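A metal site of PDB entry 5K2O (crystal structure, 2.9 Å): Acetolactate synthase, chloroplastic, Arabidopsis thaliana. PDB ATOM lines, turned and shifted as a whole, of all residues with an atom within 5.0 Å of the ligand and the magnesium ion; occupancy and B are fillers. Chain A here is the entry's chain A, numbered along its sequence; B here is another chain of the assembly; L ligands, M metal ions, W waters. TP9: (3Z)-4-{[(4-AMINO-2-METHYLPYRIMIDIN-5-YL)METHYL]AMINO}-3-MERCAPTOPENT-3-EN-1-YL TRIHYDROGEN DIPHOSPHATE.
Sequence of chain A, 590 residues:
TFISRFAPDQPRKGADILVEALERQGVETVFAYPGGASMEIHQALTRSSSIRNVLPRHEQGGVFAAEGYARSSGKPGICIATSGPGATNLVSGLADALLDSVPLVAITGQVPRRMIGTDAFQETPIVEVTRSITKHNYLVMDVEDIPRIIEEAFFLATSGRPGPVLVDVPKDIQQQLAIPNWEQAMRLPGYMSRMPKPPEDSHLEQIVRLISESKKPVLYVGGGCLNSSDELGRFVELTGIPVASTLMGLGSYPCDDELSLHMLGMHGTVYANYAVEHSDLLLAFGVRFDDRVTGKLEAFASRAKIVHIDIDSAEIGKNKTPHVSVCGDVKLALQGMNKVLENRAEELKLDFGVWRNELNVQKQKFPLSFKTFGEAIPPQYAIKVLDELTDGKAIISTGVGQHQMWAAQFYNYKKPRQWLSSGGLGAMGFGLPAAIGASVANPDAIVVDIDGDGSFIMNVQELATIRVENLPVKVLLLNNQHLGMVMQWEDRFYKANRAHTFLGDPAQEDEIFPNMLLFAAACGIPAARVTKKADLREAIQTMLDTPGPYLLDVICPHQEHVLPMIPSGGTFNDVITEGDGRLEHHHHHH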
ATOM      1  N   VAL A 400      11.998  11.379  24.615  1.00  0.00           N
ATOM      2  CA  VAL A 400      12.016  11.086  26.042  1.00  0.00           C
ATOM      3  C   VAL A 400      12.079  12.375  26.836  1.00  0.00           C
ATOM      4  O   VAL A 400      12.866  13.273  26.518  1.00  0.00           O
ATOM      5  CB  VAL A 400      13.197  10.175  26.416  1.00  0.00           C
ATOM      6  CG1 VAL A 400      13.340  10.045  27.919  1.00  0.00           C
ATOM      7  CG2 VAL A 400      13.025   8.806  25.771  1.00  0.00           C
ATOM      8  N   GLY A 401      11.235  12.470  27.858  1.00  0.00           N
ATOM      9  CA  GLY A 401      11.177  13.657  28.688  1.00  0.00           C
ATOM     10  C   GLY A 401       9.762  14.029  29.060  1.00  0.00           C
ATOM     11  O   GLY A 401       8.873  13.174  29.060  1.00  0.00           O
ATOM     12  N   GLN A 402       9.553  15.302  29.372  1.00  0.00           N
ATOM     13  CA  GLN A 402       8.234  15.793  29.760  1.00  0.00           C
ATOM     14  C   GLN A 402       7.192  15.582  28.669  1.00  0.00           C
ATOM     15  O   GLN A 402       6.082  15.115  28.951  1.00  0.00           O
ATOM     16  CB  GLN A 402       8.313  17.278  30.109  1.00  0.00           C
ATOM     17  CG  GLN A 402       9.133  17.591  31.341  1.00  0.00           C
ATOM     18  CD  GLN A 402       9.072  19.062  31.717  1.00  0.00           C
ATOM     19  OE1 GLN A 402       9.233  19.934  30.859  1.00  0.00           O
ATOM     20  NE2 GLN A 402       8.837  19.334  32.992  1.00  0.00           N
ATOM     21  N   HIS A 403       7.548  15.910  27.431  1.00  0.00           N
ATOM     22  CA  HIS A 403       6.631  15.782  26.304  1.00  0.00           C
ATOM     23  C   HIS A 403       6.163  14.341  26.147  1.00  0.00           C
ATOM     24  O   HIS A 403       5.030  14.074  25.740  1.00  0.00           O
ATOM     25  CB  HIS A 403       7.298  16.255  25.000  1.00  0.00           C
ATOM     26  CG  HIS A 403       8.412  15.374  24.542  1.00  0.00           C
ATOM     27  ND1 HIS A 403       9.677  15.411  25.084  1.00  0.00           N
ATOM     28  CD2 HIS A 403       8.443  14.406  23.587  1.00  0.00           C
ATOM     29  CE1 HIS A 403      10.437  14.518  24.492  1.00  0.00           C
ATOM     30  NE2 HIS A 403       9.719  13.897  23.576  1.00  0.00           N
ATOM     31  N   TRP A 406       3.450  13.713  28.831  1.00  0.00           N
ATOM     32  CA  TRP A 406       2.230  14.405  28.457  1.00  0.00           C
ATOM     33  C   TRP A 406       1.553  13.720  27.279  1.00  0.00           C
ATOM     34  O   TRP A 406       0.327  13.690  27.187  1.00  0.00           O
ATOM     35  CB  TRP A 406       2.528  15.868  28.129  1.00  0.00           C
ATOM     36  CG  TRP A 406       2.891  16.671  29.343  1.00  0.00           C
ATOM     37  CD1 TRP A 406       2.355  16.565  30.586  1.00  0.00           C
ATOM     38  CD2 TRP A 406       3.898  17.698  29.433  1.00  0.00           C
ATOM     39  NE1 TRP A 406       2.946  17.459  31.448  1.00  0.00           N
ATOM     40  CE2 TRP A 406       3.894  18.163  30.760  1.00  0.00           C
ATOM     41  CE3 TRP A 406       4.779  18.269  28.511  1.00  0.00           C
ATOM     42  CZ2 TRP A 406       4.756  19.175  31.196  1.00  0.00           C
ATOM     43  CZ3 TRP A 406       5.633  19.269  28.951  1.00  0.00           C
ATOM     44  CH2 TRP A 406       5.611  19.710  30.276  1.00  0.00           C
ATOM     45  N   GLY A 426      14.731   4.451  27.704  1.00  0.00           N
ATOM     46  CA  GLY A 426      14.384   5.863  27.650  1.00  0.00           C
ATOM     47  C   GLY A 426      15.371   6.675  26.841  1.00  0.00           C
ATOM     48  O   GLY A 426      15.955   7.638  27.331  1.00  0.00           O
ATOM     49  N   ALA A 427      15.543   6.290  25.579  1.00  0.00           N
ATOM     50  CA  ALA A 427      16.537   6.921  24.714  1.00  0.00           C
ATOM     51  C   ALA A 427      15.960   8.091  23.927  1.00  0.00           C
ATOM     52  O   ALA A 427      15.026   7.929  23.156  1.00  0.00           O
ATOM     53  CB  ALA A 427      17.131   5.889  23.756  1.00  0.00           C
ATOM     54  N   MET A 428      16.537   9.277  24.132  1.00  0.00           N
ATOM     55  CA  MET A 428      16.180  10.454  23.349  1.00  0.00           C
ATOM     56  C   MET A 428      16.509  10.239  21.879  1.00  0.00           C
ATOM     57  O   MET A 428      17.350   9.422  21.530  1.00  0.00           O
ATOM     58  CB  MET A 428      16.916  11.688  23.865  1.00  0.00           C
ATOM     59  CG  MET A 428      16.441  12.192  25.213  1.00  0.00           C
ATOM     60  SD  MET A 428      17.528  13.476  25.849  1.00  0.00           S
ATOM     61  CE  MET A 428      17.347  14.736  24.585  1.00  0.00           C
ATOM     62  N   GLY A 452      10.359  16.447  21.875  1.00  0.00           N
ATOM     63  CA  GLY A 452      10.923  17.569  22.612  1.00  0.00           C
ATOM     64  C   GLY A 452      12.063  18.154  21.809  1.00  0.00           C
ATOM     65  O   GLY A 452      12.608  17.479  20.933  1.00  0.00           O
ATOM     66  N   ASP A 453      12.429  19.405  22.088  1.00  0.00           N
ATOM     67  CA  ASP A 453      13.431  20.098  21.291  1.00  0.00           C
ATOM     68  C   ASP A 453      14.817  19.487  21.470  1.00  0.00           C
ATOM     69  O   ASP A 453      15.672  19.596  20.581  1.00  0.00           O
ATOM     70  CB  ASP A 453      13.461  21.585  21.628  1.00  0.00           C
ATOM     71  CG  ASP A 453      13.646  21.849  23.108  1.00  0.00           C
ATOM     72  OD1 ASP A 453      12.995  21.146  23.921  1.00  0.00           O
ATOM     73  OD2 ASP A 453      14.438  22.737  23.461  1.00  0.00           O
ATOM     74  N   GLY A 454      15.047  18.855  22.614  1.00  0.00           N
ATOM     75  CA  GLY A 454      16.307  18.171  22.852  1.00  0.00           C
ATOM     76  C   GLY A 454      16.345  16.859  22.104  1.00  0.00           C
ATOM     77  O   GLY A 454      17.316  16.541  21.415  1.00  0.00           O
ATOM     78  N   SER A 455      15.280  16.074  22.259  1.00  0.00           N
ATOM     79  CA  SER A 455      15.174  14.768  21.615  1.00  0.00           C
ATOM     80  C   SER A 455      15.147  14.887  20.096  1.00  0.00           C
ATOM     81  O   SER A 455      15.773  14.104  19.389  1.00  0.00           O
ATOM     82  CB  SER A 455      13.929  14.033  22.114  1.00  0.00           C
ATOM     83  OG  SER A 455      13.987  13.808  23.508  1.00  0.00           O
ATOM     84  N   MET A 458      18.586  15.538  18.181  1.00  0.00           N
ATOM     85  CA  MET A 458      19.587  14.474  18.229  1.00  0.00           C
ATOM     86  C   MET A 458      19.664  13.677  16.938  1.00  0.00           C
ATOM     87  O   MET A 458      20.759  13.361  16.458  1.00  0.00           O
ATOM     88  CB  MET A 458      19.304  13.520  19.383  1.00  0.00           C
ATOM     89  CG  MET A 458      19.760  14.024  20.743  1.00  0.00           C
ATOM     90  SD  MET A 458      19.913  12.689  21.937  1.00  0.00           S
ATOM     91  CE  MET A 458      20.626  13.562  23.325  1.00  0.00           C
ATOM     92  N   LEU A 478       7.009  19.906  20.806  1.00  0.00           N
ATOM     93  CA  LEU A 478       6.741  20.710  21.991  1.00  0.00           C
ATOM     94  C   LEU A 478       8.034  21.350  22.457  1.00  0.00           C
ATOM     95  O   LEU A 478       8.866  20.703  23.099  1.00  0.00           O
ATOM     96  CB  LEU A 478       6.111  19.858  23.099  1.00  0.00           C
ATOM     97  CG  LEU A 478       4.834  19.119  22.678  1.00  0.00           C
ATOM     98  CD1 LEU A 478       4.214  18.390  23.860  1.00  0.00           C
ATOM     99  CD2 LEU A 478       3.839  20.073  22.038  1.00  0.00           C
ATOM    100  N   ASN A 480      10.181  23.690  24.615  1.00  0.00           N
ATOM    101  CA  ASN A 480      10.316  24.432  25.864  1.00  0.00           C
ATOM    102  C   ASN A 480      11.716  24.990  26.062  1.00  0.00           C
ATOM    103  O   ASN A 480      12.058  25.465  27.146  1.00  0.00           O
ATOM    104  CB  ASN A 480       9.926  23.551  27.058  1.00  0.00           C
ATOM    105  CG  ASN A 480      10.748  22.273  27.142  1.00  0.00           C
ATOM    106  OD1 ASN A 480      11.724  22.099  26.419  1.00  0.00           O
ATOM    107  ND2 ASN A 480      10.356  21.381  28.044  1.00  0.00           N
ATOM    108  N   GLN A 481      12.530  24.920  25.008  1.00  0.00           N
ATOM    109  CA  GLN A 481      13.892  25.462  25.006  1.00  0.00           C
ATOM    110  C   GLN A 481      14.783  24.864  26.088  1.00  0.00           C
ATOM    111  O   GLN A 481      15.832  25.412  26.412  1.00  0.00           O
ATOM    112  CB  GLN A 481      13.855  26.978  25.152  1.00  0.00           C
ATOM    113  CG  GLN A 481      13.213  27.690  23.979  1.00  0.00           C
ATOM    114  CD  GLN A 481      14.124  27.748  22.767  1.00  0.00           C
ATOM    115  OE1 GLN A 481      14.913  28.677  22.619  1.00  0.00           O
ATOM    116  NE2 GLN A 481      14.009  26.755  21.897  1.00  0.00           N
ATOM    117  N   HIS A 482      14.365  23.725  26.650  1.00  0.00           N
ATOM    118  CA  HIS A 482      15.081  23.107  27.752  1.00  0.00           C
ATOM    119  C   HIS A 482      15.118  21.581  27.628  1.00  0.00           C
ATOM    120  O   HIS A 482      14.319  20.986  26.919  1.00  0.00           O
ATOM    121  CB  HIS A 482      14.447  23.482  29.089  1.00  0.00           C
ATOM    122  CG  HIS A 482      14.754  24.875  29.545  1.00  0.00           C
ATOM    123  ND1 HIS A 482      14.188  25.985  28.964  1.00  0.00           N
ATOM    124  CD2 HIS A 482      15.555  25.327  30.535  1.00  0.00           C
ATOM    125  CE1 HIS A 482      14.630  27.066  29.581  1.00  0.00           C
ATOM    126  NE2 HIS A 482      15.467  26.703  30.528  1.00  0.00           N
ATOM    127  N   LEU A 483      16.053  20.971  28.345  1.00  0.00           N
ATOM    128  CA  LEU A 483      15.957  19.553  28.649  1.00  0.00           C
ATOM    129  C   LEU A 483      14.966  19.430  29.803  1.00  0.00           C
ATOM    130  O   LEU A 483      15.343  19.332  30.967  1.00  0.00           O
ATOM    131  CB  LEU A 483      17.319  18.968  29.011  1.00  0.00           C
ATOM    132  CG  LEU A 483      18.337  18.984  27.876  1.00  0.00           C
ATOM    133  CD1 LEU A 483      19.705  18.531  28.356  1.00  0.00           C
ATOM    134  CD2 LEU A 483      17.869  18.112  26.722  1.00  0.00           C
ATOM    135  N   GLY A 484      13.685  19.441  29.448  1.00  0.00           N
ATOM    136  CA  GLY A 484      12.593  19.666  30.380  1.00  0.00           C
ATOM    137  C   GLY A 484      12.525  18.820  31.643  1.00  0.00           C
ATOM    138  O   GLY A 484      12.340  19.365  32.736  1.00  0.00           O
ATOM    139  N   MET A 485      12.666  17.515  31.493  1.00  0.00           N
ATOM    140  CA  MET A 485      12.534  16.608  32.635  1.00  0.00           C
ATOM    141  C   MET A 485      13.685  16.756  33.620  1.00  0.00           C
ATOM    142  O   MET A 485      13.497  16.671  34.835  1.00  0.00           O
ATOM    143  CB  MET A 485      12.436  15.150  32.150  1.00  0.00           C
ATOM    144  CG  MET A 485      12.237  14.140  33.274  1.00  0.00           C
ATOM    145  SD  MET A 485      10.748  14.407  34.249  1.00  0.00           S
ATOM    146  CE  MET A 485       9.470  14.166  33.010  1.00  0.00           C
ATOM    147  N   VAL A 486      14.885  16.996  33.098  1.00  0.00           N
ATOM    148  CA  VAL A 486      16.048  17.227  33.941  1.00  0.00           C
ATOM    149  C   VAL A 486      15.867  18.565  34.650  1.00  0.00           C
ATOM    150  O   VAL A 486      16.221  18.727  35.815  1.00  0.00           O
ATOM    151  CB  VAL A 486      17.367  17.225  33.138  1.00  0.00           C
ATOM    152  CG1 VAL A 486      18.562  17.401  34.058  1.00  0.00           C
ATOM    153  CG2 VAL A 486      17.490  15.938  32.341  1.00  0.00           C
ATOM    154  N   LEU A 503      18.675  24.871  26.312  1.00  0.00           N
ATOM    155  CA  LEU A 503      19.092  24.468  24.970  1.00  0.00           C
ATOM    156  C   LEU A 503      19.134  25.624  23.978  1.00  0.00           C
ATOM    157  O   LEU A 503      19.504  25.426  22.815  1.00  0.00           O
ATOM    158  CB  LEU A 503      18.173  23.375  24.445  1.00  0.00           C
ATOM    159  CG  LEU A 503      18.253  22.018  25.129  1.00  0.00           C
ATOM    160  CD1 LEU A 503      17.171  21.100  24.605  1.00  0.00           C
ATOM    161  CD2 LEU A 503      19.620  21.393  24.925  1.00  0.00           C
ATOM    162  N   TYR B  33      26.787  15.824  28.891  1.00  0.00           N
ATOM    163  CA  TYR B  33      25.363  15.912  28.570  1.00  0.00           C
ATOM    164  C   TYR B  33      24.551  15.312  29.715  1.00  0.00           C
ATOM    165  O   TYR B  33      24.664  14.113  30.003  1.00  0.00           O
ATOM    166  CB  TYR B  33      25.072  15.203  27.253  1.00  0.00           C
ATOM    167  CG  TYR B  33      23.753  15.563  26.619  1.00  0.00           C
ATOM    168  CD1 TYR B  33      22.568  14.961  27.029  1.00  0.00           C
ATOM    169  CD2 TYR B  33      23.678  16.516  25.604  1.00  0.00           C
ATOM    170  CE1 TYR B  33      21.359  15.289  26.459  1.00  0.00           C
ATOM    171  CE2 TYR B  33      22.474  16.845  25.020  1.00  0.00           C
ATOM    172  CZ  TYR B  33      21.321  16.238  25.450  1.00  0.00           C
ATOM    173  OH  TYR B  33      20.117  16.567  24.867  1.00  0.00           O
ATOM    174  N   PRO B  34      23.731  16.133  30.370  1.00  0.00           N
ATOM    175  CA  PRO B  34      23.075  15.743  31.630  1.00  0.00           C
ATOM    176  C   PRO B  34      21.985  14.691  31.467  1.00  0.00           C
ATOM    177  O   PRO B  34      21.353  14.572  30.415  1.00  0.00           O
ATOM    178  CB  PRO B  34      22.465  17.057  32.128  1.00  0.00           C
ATOM    179  CG  PRO B  34      22.244  17.853  30.892  1.00  0.00           C
ATOM    180  CD  PRO B  34      23.374  17.513  29.975  1.00  0.00           C
ATOM    181  N   GLY B  35      21.776  13.942  32.543  1.00  0.00           N
ATOM    182  CA  GLY B  35      20.691  12.982  32.633  1.00  0.00           C
ATOM    183  C   GLY B  35      20.483  12.690  34.100  1.00  0.00           C
ATOM    184  O   GLY B  35      21.311  13.046  34.933  1.00  0.00           O
ATOM    185  N   GLY B  36      19.371  12.039  34.429  1.00  0.00           N
ATOM    186  CA  GLY B  36      19.013  11.772  35.816  1.00  0.00           C
ATOM    187  C   GLY B  36      20.098  11.077  36.616  1.00  0.00           C
ATOM    188  O   GLY B  36      20.285  11.362  37.800  1.00  0.00           O
ATOM    189  N   GLU B  59      25.529  12.822  22.678  1.00  0.00           N
ATOM    190  CA  GLU B  59      26.706  12.315  23.383  1.00  0.00           C
ATOM    191  C   GLU B  59      27.785  11.804  22.434  1.00  0.00           C
ATOM    192  O   GLU B  59      28.962  11.785  22.800  1.00  0.00           O
ATOM    193  CB  GLU B  59      26.314  11.211  24.355  1.00  0.00           C
ATOM    194  CG  GLU B  59      25.554  11.696  25.574  1.00  0.00           C
ATOM    195  CD  GLU B  59      24.052  11.607  25.407  1.00  0.00           C
ATOM    196  OE1 GLU B  59      23.578  11.445  24.270  1.00  0.00           O
ATOM    197  OE2 GLU B  59      23.345  11.696  26.437  1.00  0.00           O
ATOM    198  N   THR B  82      25.103  10.423  30.931  1.00  0.00           N
ATOM    199  CA  THR B  82      24.266   9.758  31.917  1.00  0.00           C
ATOM    200  C   THR B  82      24.230   8.250  31.660  1.00  0.00           C
ATOM    201  O   THR B  82      24.856   7.761  30.715  1.00  0.00           O
ATOM    202  CB  THR B  82      22.840  10.322  31.910  1.00  0.00           C
ATOM    203  OG1 THR B  82      22.169   9.960  33.120  1.00  0.00           O
ATOM    204  CG2 THR B  82      22.056   9.822  30.710  1.00  0.00           C
ATOM    205  N   PRO B  85      21.092   5.192  27.762  1.00  0.00           N
ATOM    206  CA  PRO B  85      21.148   5.772  26.415  1.00  0.00           C
ATOM    207  C   PRO B  85      22.242   6.825  26.282  1.00  0.00           C
ATOM    208  O   PRO B  85      22.728   7.064  25.180  1.00  0.00           O
ATOM    209  CB  PRO B  85      19.758   6.393  26.258  1.00  0.00           C
ATOM    210  CG  PRO B  85      19.306   6.668  27.645  1.00  0.00           C
ATOM    211  CD  PRO B  85      19.848   5.533  28.467  1.00  0.00           C
ATOM    212  N   GLY B  86      22.604   7.455  27.400  1.00  0.00           N
ATOM    213  CA  GLY B  86      23.727   8.371  27.406  1.00  0.00           C
ATOM    214  C   GLY B  86      25.015   7.611  27.170  1.00  0.00           C
ATOM    215  O   GLY B  86      25.811   7.974  26.299  1.00  0.00           O
ATOM    216  N   ASN B  89      25.520   5.988  23.726  1.00  0.00           N
ATOM    217  CA  ASN B  89      25.773   6.988  22.700  1.00  0.00           C
ATOM    218  C   ASN B  89      27.248   7.376  22.618  1.00  0.00           C
ATOM    219  O   ASN B  89      27.654   8.108  21.711  1.00  0.00           O
ATOM    220  CB  ASN B  89      24.923   8.230  22.946  1.00  0.00           C
ATOM    221  CG  ASN B  89      23.576   8.169  22.256  1.00  0.00           C
ATOM    222  OD1 ASN B  89      23.290   7.227  21.519  1.00  0.00           O
ATOM    223  ND2 ASN B  89      22.745   9.181  22.478  1.00  0.00           N
ATOM    224  N   GLN B 122      16.950   3.075  32.588  1.00  0.00           N
ATOM    225  CA  GLN B 122      18.160   3.570  31.936  1.00  0.00           C
ATOM    226  C   GLN B 122      19.421   2.865  32.424  1.00  0.00           C
ATOM    227  O   GLN B 122      20.451   3.501  32.663  1.00  0.00           O
ATOM    228  CB  GLN B 122      18.288   5.084  32.154  1.00  0.00           C
ATOM    229  CG  GLN B 122      17.090   5.871  31.666  1.00  0.00           C
ATOM    230  CD  GLN B 122      17.364   7.360  31.574  1.00  0.00           C
ATOM    231  OE1 GLN B 122      17.903   7.960  32.501  1.00  0.00           O
ATOM    232  NE2 GLN B 122      16.994   7.957  30.448  1.00  0.00           N
HETATM  233  N1' TP9 L   1      20.607  11.189  26.406  1.00  0.00           N
HETATM  234  C2' TP9 L   1      19.740  10.339  25.896  1.00  0.00           C
HETATM  235  CM2 TP9 L   1      20.058   9.696  24.558  1.00  0.00           C
HETATM  236  N3' TP9 L   1      18.616  10.021  26.510  1.00  0.00           N
HETATM  237  C4' TP9 L   1      18.294  10.562  27.693  1.00  0.00           C
HETATM  238  N4' TP9 L   1      17.088  10.209  28.334  1.00  0.00           N
HETATM  239  C5' TP9 L   1      19.194  11.479  28.282  1.00  0.00           C
HETATM  240  C6' TP9 L   1      20.375  11.787  27.590  1.00  0.00           C
HETATM  241  C7' TP9 L   1      18.926  12.151  29.618  1.00  0.00           C
HETATM  242  N3  TP9 L   1      17.606  12.673  29.711  1.00  0.00           N
HETATM  243  S1  TP9 L   1      14.573  13.435  29.485  1.00  0.00           S
HETATM  244  C5  TP9 L   1      15.993  14.413  29.133  1.00  0.00           C
HETATM  245  C4  TP9 L   1      17.265  13.984  29.272  1.00  0.00           C
HETATM  246  CM4 TP9 L   1      18.500  14.809  28.965  1.00  0.00           C
HETATM  247  C6  TP9 L   1      15.566  15.791  28.649  1.00  0.00           C
HETATM  248  C7  TP9 L   1      15.063  15.766  27.221  1.00  0.00           C
HETATM  249  O7  TP9 L   1      14.495  17.018  26.924  1.00  0.00           O
HETATM  250  PA  TP9 L   1      13.515  17.133  25.674  1.00  0.00           P
HETATM  251  O1A TP9 L   1      13.599  18.529  25.104  1.00  0.00           O
HETATM  252  O2A TP9 L   1      13.901  16.126  24.628  1.00  0.00           O
HETATM  253  O3A TP9 L   1      12.029  16.854  26.156  1.00  0.00           O
HETATM  254  PB  TP9 L   1      11.335  17.655  27.324  1.00  0.00           P
HETATM  255  O1B TP9 L   1       9.845  17.650  27.092  1.00  0.00           O
HETATM  256  O2B TP9 L   1      11.635  17.005  28.647  1.00  0.00           O
HETATM  257  O3B TP9 L   1      11.839  19.072  27.326  1.00  0.00           O
HETATM  258 MG    MG M   1      12.743  20.236  25.907  1.00  0.00          MG
HETATM  259  O   HOH W   1       8.112  19.349  26.143  1.00  0.00           O
HETATM  260  O   HOH W   2      10.790  19.827  24.898  1.00  0.00           O
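Water W2 lies within hydrogen-bond range of the backbone carbonyl oxygen of Leu 478 (2.8 Å), an oxygen (O1B) of the ligand (3.2 Å) and the backbone NH of Asp 453 (3.3 Å).
Water W1 bridges O1B of the ligand (2.6 Å) and O of Leu 478 (3.4 Å).
The backbone NH of Asp 453 lies close to an oxygen (O1A) of the ligand, at 3.4 Å.
N of Ser 455 is in hydrogen-bond range of O2A of the ligand, at 2.7 Å.
The side-chain hydroxyl (OG) of Ser 455 is in hydrogen-bond range of an oxygen (O2A) of the ligand (2.6 Å).
OE2 of Glu 59 of chain B lies within hydrogen-bond range of N1' of the ligand (2.8 Å).
The backbone NH of Gln 402 is in hydrogen-bond range of an oxygen (O2B) of the ligand (2.8 Å).
An oxygen (O2B) of the ligand lies within hydrogen-bond range of the backbone NH (N) of Gly 484 (3.3 Å).
O1A of the ligand lies close to N of Gly 454, 2.9 Å away.
An oxygen (O1B) of the ligand is in hydrogen-bond range of the backbone NH of His 403, 2.9 Å away.
A ring nitrogen (ND1) of His 403 lies within hydrogen-bond range of an oxygen (O3A) of the ligand, 3.0 Å away.
N4' of the ligand lies within hydrogen-bond range of O of Gly 426 (3.0 Å).
The backbone NH (N) of Met 485 is in hydrogen-bond range of an oxygen (O2B) of the ligand (3.1 Å).
The side-chain amide nitrogen (NE2) of Gln 122 of chain B sits close to a nitrogen (N4') of the ligand, 3.1 Å away.
The backbone NH of Met 428 lies within hydrogen-bond range of a nitrogen (N3') of the ligand (3.2 Å).
O of Val 400 sits close to S1 of the ligand, at 3.4 Å.
Merely in contact with the magnesium ion: Gly 484 (3.7 Å).
Four residues have an atom within 4 Å of the magnesium ion: Asp 453, Asn 480, His 482 and Gly 484.
Merely in contact with the ligand: Gly 401, Gly 452, Met 458, Leu 483, Val 486, Tyr 33 of chain B, Pro 34 of chain B, Gly 35 of chain B, Pro 85 of chain B and Asn 89 of chain B.
Along chain A the residues within 4 Å of the ligand span positions 400 to 486.
The magnesium ion is bound by O of His 482 (2.0 Å).
An oxygen (O3B) of the ligand is bound to the magnesium ion (2.0 Å).
O1A of the ligand is bound to the magnesium ion (2.1 Å).
The side-chain amide oxygen (OD1) of Asn 480 is bound to the magnesium ion (2.2 Å).
The magnesium ion is bound by the side-chain carboxylate (OD1) of Asp 453, 2.2 Å away.
Water W2 is bound to the magnesium ion (2.2 Å).
The magnesium ion has six donor atoms within binding distance.
The side-chain amide oxygen (OE1) of Gln 402 sits at hydrogen-bond distance from the side-chain amide nitrogen (ND2) of Asn 480, 3.4 Å away.
The side-chain carboxylate of Asp 453 sits close to the backbone NH of Gln 481 (3.3 Å).
The side-chain hydroxyl of Ser 455 is in hydrogen-bond range of the backbone carbonyl oxygen of Val 400, at 3.3 Å.
OE1 of Glu 59 of chain B is in hydrogen-bond range of ND2 of Asn 89 of chain B, at 3.0 Å.
A ring nitrogen (NE2) of His 403 sits at hydrogen-bond distance from the backbone NH (N) of Gly 452, at 3.1 Å.
The backbone carbonyl oxygen of Gly 426 is in hydrogen-bond range of the side-chain amide nitrogen of Gln 122 of chain B, 3.3 Å away.
The side-chain amide nitrogen (ND2) of Asn 89 of chain B lies close to the backbone carbonyl oxygen (O) of Pro 85 of chain B (3.4 Å).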
